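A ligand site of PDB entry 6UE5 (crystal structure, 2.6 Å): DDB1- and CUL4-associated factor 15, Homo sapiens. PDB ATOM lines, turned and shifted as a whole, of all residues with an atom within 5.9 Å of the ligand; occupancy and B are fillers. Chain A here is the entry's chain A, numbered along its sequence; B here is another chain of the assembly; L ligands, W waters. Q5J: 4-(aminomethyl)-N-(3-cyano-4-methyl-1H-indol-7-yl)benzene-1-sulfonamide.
A nitrogen (N2) of the ligand lies within hydrogen-bond range of the backbone carbonyl oxygen of Phe 232, at 3.1 Å.
The backbone NH (N) of Ala 235 is in hydrogen-bond range of an oxygen (O1) of the ligand (3.0 Å).
The backbone NH (N) of Phe 236 lies within hydrogen-bond range of an oxygen (O2) of the ligand (3.2 Å).
N of Gln 233 is in hydrogen-bond range of OE1 of Gln 237 (2.8 Å).
OE1 of Gln 233 is in hydrogen-bond range of OG1 of Thr 231 (3.5 Å).
The guanidinium group of Arg 553 is in hydrogen-bond range of the backbone carbonyl oxygen of Gly 21 of chain B (2.8 Å).
The backbone NH (N) of Met 18 of chain B sits at hydrogen-bond distance from the side-chain hydroxyl (OG1) of Thr 15 of chain B (3.1 Å).
The backbone carbonyl oxygen (O) of Ile 479 sits at hydrogen-bond distance from the side-chain amide nitrogen (NE2) of Gln 233 (2.9 Å).
N of Asp 17 of chain B is in hydrogen-bond range of OG1 of Thr 15 of chain B (3.3 Å).
An oxygen (O1) of the ligand lies close to the backbone nitrogen of Pro 234 (3.4 Å).
Thr 231 touches the ligand (CG2 to C9, 3.8 Å).
Gln 233 touches the ligand.
Val 478 touches the ligand (CG1 to C7, 3.8 Å).
Arg 553 touches the ligand (CB to N1, 3.5 Å).
CB of Cys 556 touches C7 of the ligand, 3.8 Å away.
N of Val 557 touches C7 of the ligand, 3.7 Å away.
CD2 of Leu 564 touches C17 of the ligand, 3.7 Å away.
CG2 of Thr 15 of chain B touches C16 of the ligand (3.9 Å).
Asp 17 of chain B touches the ligand (O to C10, 3.4 Å).
CA of Met 18 of chain B touches C10 of the ligand, at 3.5 Å.
Hydrophobic or aromatic side chains within 4 Å of the ligand: Pro 234, Ala 235, Phe 236, Val 478, Val 557, Leu 564 and Met 18 of chain B.
Within 4 Å of the ligand: Thr 231, Phe 232, Gln 233, Pro 234, Ala 235, Phe 236, Val 478, Arg 553, Cys 556, Val 557, Leu 564, Thr 15 of chain B, Asp 17 of chain B and Met 18 of chain B.
Water W2 lies within hydrogen-bond range of OG1 of Thr 15 of chain B (2.6 Å) and N3 of the ligand (2.7 Å).
Water W1 bridges O of Asn 13 of chain B (3.3 Å) and N4 of the ligand (3.3 Å).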
ATOM      1  N   THR A 231     -20.498 -22.868   9.844  1.00  0.00           N
ATOM      2  CA  THR A 231     -19.836 -23.569   8.757  1.00  0.00           C
ATOM      3  C   THR A 231     -19.339 -22.574   7.734  1.00  0.00           C
ATOM      4  O   THR A 231     -19.923 -21.503   7.574  1.00  0.00           O
ATOM      5  CB  THR A 231     -20.790 -24.587   8.108  1.00  0.00           C
ATOM      6  OG1 THR A 231     -22.013 -23.937   7.741  1.00  0.00           O
ATOM      7  CG2 THR A 231     -21.081 -25.776   9.004  1.00  0.00           C
ATOM      8  N   PHE A 232     -18.244 -22.945   7.053  1.00  0.00           N
ATOM      9  CA  PHE A 232     -17.638 -22.134   6.003  1.00  0.00           C
ATOM     10  C   PHE A 232     -18.143 -22.631   4.652  1.00  0.00           C
ATOM     11  O   PHE A 232     -17.860 -23.766   4.258  1.00  0.00           O
ATOM     12  CB  PHE A 232     -16.097 -22.161   6.091  1.00  0.00           C
ATOM     13  CG  PHE A 232     -15.536 -21.725   7.423  1.00  0.00           C
ATOM     14  CD1 PHE A 232     -15.322 -20.382   7.707  1.00  0.00           C
ATOM     15  CD2 PHE A 232     -15.230 -22.664   8.402  1.00  0.00           C
ATOM     16  CE1 PHE A 232     -14.822 -19.979   8.950  1.00  0.00           C
ATOM     17  CE2 PHE A 232     -14.730 -22.260   9.645  1.00  0.00           C
ATOM     18  CZ  PHE A 232     -14.537 -20.917   9.909  1.00  0.00           C
ATOM     19  N   GLN A 233     -18.973 -21.813   3.996  1.00  0.00           N
ATOM     20  CA  GLN A 233     -19.578 -22.133   2.711  1.00  0.00           C
ATOM     21  C   GLN A 233     -19.174 -21.099   1.644  1.00  0.00           C
ATOM     22  O   GLN A 233     -20.014 -20.285   1.252  1.00  0.00           O
ATOM     23  CB  GLN A 233     -21.116 -22.218   2.862  1.00  0.00           C
ATOM     24  CG  GLN A 233     -21.550 -23.068   4.048  1.00  0.00           C
ATOM     25  CD  GLN A 233     -23.040 -23.059   4.243  1.00  0.00           C
ATOM     26  OE1 GLN A 233     -23.575 -22.319   5.079  1.00  0.00           O
ATOM     27  NE2 GLN A 233     -23.742 -23.874   3.472  1.00  0.00           N
ATOM     28  N   PRO A 234     -17.902 -21.076   1.176  1.00  0.00           N
ATOM     29  CA  PRO A 234     -17.491 -20.038   0.213  1.00  0.00           C
ATOM     30  C   PRO A 234     -18.228 -20.021  -1.119  1.00  0.00           C
ATOM     31  O   PRO A 234     -18.388 -18.927  -1.665  1.00  0.00           O
ATOM     32  CB  PRO A 234     -15.989 -20.292   0.019  1.00  0.00           C
ATOM     33  CG  PRO A 234     -15.783 -21.684   0.428  1.00  0.00           C
ATOM     34  CD  PRO A 234     -16.756 -21.926   1.536  1.00  0.00           C
ATOM     35  N   ALA A 235     -18.666 -21.195  -1.645  1.00  0.00           N
ATOM     36  CA  ALA A 235     -19.406 -21.252  -2.925  1.00  0.00           C
ATOM     37  C   ALA A 235     -20.758 -20.536  -2.832  1.00  0.00           C
ATOM     38  O   ALA A 235     -21.151 -19.875  -3.791  1.00  0.00           O
ATOM     39  CB  ALA A 235     -19.593 -22.688  -3.391  1.00  0.00           C
ATOM     40  N   PHE A 236     -21.437 -20.620  -1.658  1.00  0.00           N
ATOM     41  CA  PHE A 236     -22.710 -19.934  -1.444  1.00  0.00           C
ATOM     42  C   PHE A 236     -22.494 -18.503  -1.007  1.00  0.00           C
ATOM     43  O   PHE A 236     -23.134 -17.616  -1.573  1.00  0.00           O
ATOM     44  CB  PHE A 236     -23.601 -20.664  -0.434  1.00  0.00           C
ATOM     45  CG  PHE A 236     -24.231 -21.928  -0.958  1.00  0.00           C
ATOM     46  CD1 PHE A 236     -24.697 -22.004  -2.266  1.00  0.00           C
ATOM     47  CD2 PHE A 236     -24.396 -23.033  -0.138  1.00  0.00           C
ATOM     48  CE1 PHE A 236     -25.265 -23.177  -2.749  1.00  0.00           C
ATOM     49  CE2 PHE A 236     -24.968 -24.199  -0.616  1.00  0.00           C
ATOM     50  CZ  PHE A 236     -25.390 -24.272  -1.930  1.00  0.00           C
ATOM     51  N   GLN A 237     -21.591 -18.271  -0.012  1.00  0.00           N
ATOM     52  CA  GLN A 237     -21.276 -16.955   0.553  1.00  0.00           C
ATOM     53  C   GLN A 237     -20.913 -15.892  -0.493  1.00  0.00           C
ATOM     54  O   GLN A 237     -21.195 -14.714  -0.271  1.00  0.00           O
ATOM     55  CB  GLN A 237     -20.184 -17.048   1.628  1.00  0.00           C
ATOM     56  CG  GLN A 237     -20.623 -17.738   2.914  1.00  0.00           C
ATOM     57  CD  GLN A 237     -19.460 -17.934   3.864  1.00  0.00           C
ATOM     58  OE1 GLN A 237     -18.908 -19.020   3.976  1.00  0.00           O
ATOM     59  NE2 GLN A 237     -19.085 -16.882   4.563  1.00  0.00           N
ATOM     60  N   VAL A 478     -27.355 -22.792   8.280  1.00  0.00           N
ATOM     61  CA  VAL A 478     -26.643 -23.307   7.116  1.00  0.00           C
ATOM     62  C   VAL A 478     -27.348 -22.798   5.855  1.00  0.00           C
ATOM     63  O   VAL A 478     -28.566 -22.832   5.790  1.00  0.00           O
ATOM     64  CB  VAL A 478     -26.551 -24.859   7.131  1.00  0.00           C
ATOM     65  CG1 VAL A 478     -25.906 -25.414   5.862  1.00  0.00           C
ATOM     66  CG2 VAL A 478     -25.809 -25.368   8.363  1.00  0.00           C
ATOM     67  N   ILE A 479     -26.572 -22.330   4.856  1.00  0.00           N
ATOM     68  CA  ILE A 479     -27.118 -21.864   3.583  1.00  0.00           C
ATOM     69  C   ILE A 479     -27.358 -23.077   2.659  1.00  0.00           C
ATOM     70  O   ILE A 479     -26.503 -23.970   2.567  1.00  0.00           O
ATOM     71  CB  ILE A 479     -26.218 -20.792   2.898  1.00  0.00           C
ATOM     72  CG1 ILE A 479     -25.872 -19.643   3.874  1.00  0.00           C
ATOM     73  CG2 ILE A 479     -26.835 -20.265   1.589  1.00  0.00           C
ATOM     74  CD1 ILE A 479     -24.832 -18.655   3.388  1.00  0.00           C
ATOM     75  N   LEU A 480     -28.509 -23.106   1.987  1.00  0.00           N
ATOM     76  CA  LEU A 480     -28.894 -24.173   1.074  1.00  0.00           C
ATOM     77  C   LEU A 480     -28.748 -23.752  -0.375  1.00  0.00           C
ATOM     78  O   LEU A 480     -28.324 -24.565  -1.200  1.00  0.00           O
ATOM     79  CB  LEU A 480     -30.313 -24.675   1.344  1.00  0.00           C
ATOM     80  CG  LEU A 480     -30.566 -25.290   2.726  1.00  0.00           C
ATOM     81  CD1 LEU A 480     -32.021 -25.590   2.917  1.00  0.00           C
ATOM     82  CD2 LEU A 480     -29.719 -26.536   2.946  1.00  0.00           C
ATOM     83  N   ARG A 553     -26.246 -31.213  10.175  1.00  0.00           N
ATOM     84  CA  ARG A 553     -25.350 -30.766   9.111  1.00  0.00           C
ATOM     85  C   ARG A 553     -25.210 -31.813   8.015  1.00  0.00           C
ATOM     86  O   ARG A 553     -25.087 -31.444   6.852  1.00  0.00           O
ATOM     87  CB  ARG A 553     -24.003 -30.311   9.656  1.00  0.00           C
ATOM     88  CG  ARG A 553     -24.117 -28.994  10.378  1.00  0.00           C
ATOM     89  CD  ARG A 553     -22.838 -28.668  11.080  1.00  0.00           C
ATOM     90  NE  ARG A 553     -22.915 -27.352  11.694  1.00  0.00           N
ATOM     91  CZ  ARG A 553     -21.895 -26.763  12.304  1.00  0.00           C
ATOM     92  NH1 ARG A 553     -20.711 -27.327  12.378  1.00  0.00           N
ATOM     93  NH2 ARG A 553     -22.070 -25.543  12.832  1.00  0.00           N
ATOM     94  N   LYS A 554     -25.328 -33.113   8.374  1.00  0.00           N
ATOM     95  CA  LYS A 554     -25.300 -34.194   7.392  1.00  0.00           C
ATOM     96  C   LYS A 554     -26.504 -34.103   6.482  1.00  0.00           C
ATOM     97  O   LYS A 554     -26.343 -34.281   5.276  1.00  0.00           O
ATOM     98  CB  LYS A 554     -25.221 -35.558   8.054  1.00  0.00           C
ATOM     99  CG  LYS A 554     -23.786 -36.003   8.341  1.00  0.00           C
ATOM    100  CD  LYS A 554     -23.747 -37.138   9.356  1.00  0.00           C
ATOM    101  CE  LYS A 554     -24.224 -38.473   8.816  1.00  0.00           C
ATOM    102  NZ  LYS A 554     -24.327 -39.498   9.878  1.00  0.00           N
ATOM    103  N   CYS A 556     -28.123 -31.351   5.667  1.00  0.00           N
ATOM    104  CA  CYS A 556     -27.897 -30.163   4.837  1.00  0.00           C
ATOM    105  C   CYS A 556     -27.016 -30.539   3.655  1.00  0.00           C
ATOM    106  O   CYS A 556     -27.331 -30.182   2.517  1.00  0.00           O
ATOM    107  CB  CYS A 556     -27.279 -29.015   5.633  1.00  0.00           C
ATOM    108  SG  CYS A 556     -28.339 -28.370   6.956  1.00  0.00           S
ATOM    109  N   VAL A 557     -25.929 -31.321   3.935  1.00  0.00           N
ATOM    110  CA  VAL A 557     -24.997 -31.835   2.910  1.00  0.00           C
ATOM    111  C   VAL A 557     -25.784 -32.751   1.969  1.00  0.00           C
ATOM    112  O   VAL A 557     -25.641 -32.606   0.759  1.00  0.00           O
ATOM    113  CB  VAL A 557     -23.709 -32.511   3.483  1.00  0.00           C
ATOM    114  CG1 VAL A 557     -22.762 -32.943   2.364  1.00  0.00           C
ATOM    115  CG2 VAL A 557     -22.967 -31.579   4.440  1.00  0.00           C
ATOM    116  N   VAL A 560     -28.169 -30.419  -0.312  1.00  0.00           N
ATOM    117  CA  VAL A 560     -27.379 -29.693  -1.309  1.00  0.00           C
ATOM    118  C   VAL A 560     -26.899 -30.628  -2.429  1.00  0.00           C
ATOM    119  O   VAL A 560     -27.103 -30.302  -3.601  1.00  0.00           O
ATOM    120  CB  VAL A 560     -26.226 -28.858  -0.687  1.00  0.00           C
ATOM    121  CG1 VAL A 560     -25.249 -28.348  -1.751  1.00  0.00           C
ATOM    122  CG2 VAL A 560     -26.786 -27.686   0.115  1.00  0.00           C
ATOM    123  N   MET A 561     -26.320 -31.789  -2.052  1.00  0.00           N
ATOM    124  CA  MET A 561     -25.825 -32.795  -3.006  1.00  0.00           C
ATOM    125  C   MET A 561     -26.959 -33.347  -3.844  1.00  0.00           C
ATOM    126  O   MET A 561     -26.786 -33.504  -5.052  1.00  0.00           O
ATOM    127  CB  MET A 561     -25.071 -33.942  -2.302  1.00  0.00           C
ATOM    128  CG  MET A 561     -23.764 -33.523  -1.657  1.00  0.00           C
ATOM    129  SD  MET A 561     -22.520 -32.818  -2.756  1.00  0.00           S
ATOM    130  CE  MET A 561     -21.235 -32.635  -1.639  1.00  0.00           C
ATOM    131  N   LEU A 564     -28.069 -30.747  -6.537  1.00  0.00           N
ATOM    132  CA  LEU A 564     -26.910 -30.168  -7.188  1.00  0.00           C
ATOM    133  C   LEU A 564     -26.995 -30.181  -8.715  1.00  0.00           C
ATOM    134  O   LEU A 564     -27.095 -31.241  -9.332  1.00  0.00           O
ATOM    135  CB  LEU A 564     -25.610 -30.804  -6.687  1.00  0.00           C
ATOM    136  CG  LEU A 564     -24.300 -30.159  -7.115  1.00  0.00           C
ATOM    137  CD1 LEU A 564     -24.229 -28.674  -6.730  1.00  0.00           C
ATOM    138  CD2 LEU A 564     -23.146 -30.925  -6.548  1.00  0.00           C
ATOM    139  N   ASN B  13     -17.505 -35.145  -4.201  1.00  0.00           N
ATOM    140  CA  ASN B  13     -17.945 -33.754  -4.125  1.00  0.00           C
ATOM    141  C   ASN B  13     -17.951 -33.183  -2.702  1.00  0.00           C
ATOM    142  O   ASN B  13     -18.076 -31.965  -2.539  1.00  0.00           O
ATOM    143  CB  ASN B  13     -19.289 -33.579  -4.818  1.00  0.00           C
ATOM    144  CG  ASN B  13     -19.222 -33.833  -6.305  1.00  0.00           C
ATOM    145  OD1 ASN B  13     -18.173 -34.188  -6.868  1.00  0.00           O
ATOM    146  ND2 ASN B  13     -20.348 -33.647  -6.978  1.00  0.00           N
ATOM    147  N   THR B  15     -16.538 -31.713   0.504  1.00  0.00           N
ATOM    148  CA  THR B  15     -15.359 -30.889   0.712  1.00  0.00           C
ATOM    149  C   THR B  15     -14.824 -31.021   2.138  1.00  0.00           C
ATOM    150  O   THR B  15     -15.500 -31.562   3.013  1.00  0.00           O
ATOM    151  CB  THR B  15     -15.695 -29.430   0.429  1.00  0.00           C
ATOM    152  OG1 THR B  15     -16.373 -28.932   1.568  1.00  0.00           O
ATOM    153  CG2 THR B  15     -16.529 -29.239  -0.850  1.00  0.00           C
ATOM    154  N   ASP B  17     -14.331 -28.422   4.078  1.00  0.00           N
ATOM    155  CA  ASP B  17     -15.198 -27.529   4.864  1.00  0.00           C
ATOM    156  C   ASP B  17     -16.435 -28.271   5.366  1.00  0.00           C
ATOM    157  O   ASP B  17     -16.838 -28.043   6.498  1.00  0.00           O
ATOM    158  CB  ASP B  17     -15.591 -26.271   4.075  1.00  0.00           C
ATOM    159  CG  ASP B  17     -14.413 -25.384   3.708  1.00  0.00           C
ATOM    160  OD1 ASP B  17     -13.521 -25.206   4.571  1.00  0.00           O
ATOM    161  OD2 ASP B  17     -14.397 -24.855   2.569  1.00  0.00           O
ATOM    162  N   MET B  18     -16.980 -29.204   4.552  1.00  0.00           N
ATOM    163  CA  MET B  18     -18.122 -30.039   4.954  1.00  0.00           C
ATOM    164  C   MET B  18     -17.694 -31.001   6.040  1.00  0.00           C
ATOM    165  O   MET B  18     -18.399 -31.120   7.037  1.00  0.00           O
ATOM    166  CB  MET B  18     -18.741 -30.775   3.764  1.00  0.00           C
ATOM    167  CG  MET B  18     -19.477 -29.869   2.831  1.00  0.00           C
ATOM    168  SD  MET B  18     -19.779 -30.709   1.271  1.00  0.00           S
ATOM    169  CE  MET B  18     -20.431 -29.392   0.334  1.00  0.00           C
ATOM    170  N   LEU B  19     -16.496 -31.617   5.876  1.00  0.00           N
ATOM    171  CA  LEU B  19     -15.903 -32.543   6.853  1.00  0.00           C
ATOM    172  C   LEU B  19     -15.709 -31.874   8.185  1.00  0.00           C
ATOM    173  O   LEU B  19     -16.049 -32.470   9.210  1.00  0.00           O
ATOM    174  CB  LEU B  19     -14.587 -33.147   6.344  1.00  0.00           C
ATOM    175  CG  LEU B  19     -14.712 -34.249   5.315  1.00  0.00           C
ATOM    176  CD1 LEU B  19     -13.389 -34.524   4.675  1.00  0.00           C
ATOM    177  CD2 LEU B  19     -15.266 -35.536   5.931  1.00  0.00           C
ATOM    178  N   GLY B  21     -17.390 -29.165   9.281  1.00  0.00           N
ATOM    179  CA  GLY B  21     -18.754 -28.918   9.739  1.00  0.00           C
ATOM    180  C   GLY B  21     -19.405 -30.083  10.449  1.00  0.00           C
ATOM    181  O   GLY B  21     -20.077 -29.872  11.462  1.00  0.00           O
ATOM    182  N   ILE B  22     -19.176 -31.311   9.965  1.00  0.00           N
ATOM    183  CA  ILE B  22     -19.769 -32.517  10.563  1.00  0.00           C
ATOM    184  C   ILE B  22     -19.038 -32.954  11.860  1.00  0.00           C
ATOM    185  O   ILE B  22     -19.692 -33.361  12.816  1.00  0.00           O
ATOM    186  CB  ILE B  22     -19.886 -33.675   9.525  1.00  0.00           C
ATOM    187  CG1 ILE B  22     -20.582 -33.220   8.233  1.00  0.00           C
ATOM    188  CG2 ILE B  22     -20.605 -34.900  10.120  1.00  0.00           C
ATOM    189  CD1 ILE B  22     -20.369 -34.119   7.035  1.00  0.00           C
HETATM  190  C1  Q5J L   1     -23.201 -26.693   1.923  1.00  0.00           C
HETATM  191  C2  Q5J L   1     -22.188 -25.983   1.263  1.00  0.00           C
HETATM  192  C3  Q5J L   1     -20.921 -25.830   1.872  1.00  0.00           C
HETATM  193  O1  Q5J L   1     -18.427 -23.954  -0.464  1.00  0.00           O
HETATM  194  O2  Q5J L   1     -20.907 -23.373  -0.218  1.00  0.00           O
HETATM  195  C11 Q5J L   1     -20.227 -25.628  -1.499  1.00  0.00           C
HETATM  196  C12 Q5J L   1     -21.507 -25.647  -2.100  1.00  0.00           C
HETATM  197  C13 Q5J L   1     -21.808 -26.642  -3.067  1.00  0.00           C
HETATM  198  C14 Q5J L   1     -20.829 -27.599  -3.421  1.00  0.00           C
HETATM  199  C15 Q5J L   1     -19.548 -27.566  -2.800  1.00  0.00           C
HETATM  200  C16 Q5J L   1     -19.237 -26.591  -1.835  1.00  0.00           C
HETATM  201  C17 Q5J L   1     -21.173 -28.643  -4.477  1.00  0.00           C
HETATM  202  C10 Q5J L   1     -19.815 -26.964   5.158  1.00  0.00           C
HETATM  203  C4  Q5J L   1     -20.695 -26.362   3.157  1.00  0.00           C
HETATM  204  C5  Q5J L   1     -21.705 -27.093   3.873  1.00  0.00           C
HETATM  205  C6  Q5J L   1     -22.973 -27.249   3.206  1.00  0.00           C
HETATM  206  C7  Q5J L   1     -24.133 -28.032   3.800  1.00  0.00           C
HETATM  207  C8  Q5J L   1     -21.090 -27.454   5.149  1.00  0.00           C
HETATM  208  C9  Q5J L   1     -21.722 -28.186   6.176  1.00  0.00           C
HETATM  209  N1  Q5J L   1     -22.240 -28.785   7.018  1.00  0.00           N
HETATM  210  N2  Q5J L   1     -19.584 -26.310   3.964  1.00  0.00           N
HETATM  211  N3  Q5J L   1     -19.887 -25.179   1.200  1.00  0.00           N
HETATM  212  N4  Q5J L   1     -20.053 -29.444  -4.962  1.00  0.00           N
HETATM  213  S1  Q5J L   1     -19.823 -24.365  -0.296  1.00  0.00           S
HETATM  214  O   HOH W   1     -16.764 -29.707  -4.520  1.00  0.00           O
HETATM  215  O   HOH W   2     -17.625 -26.635   1.448  1.00  0.00           O
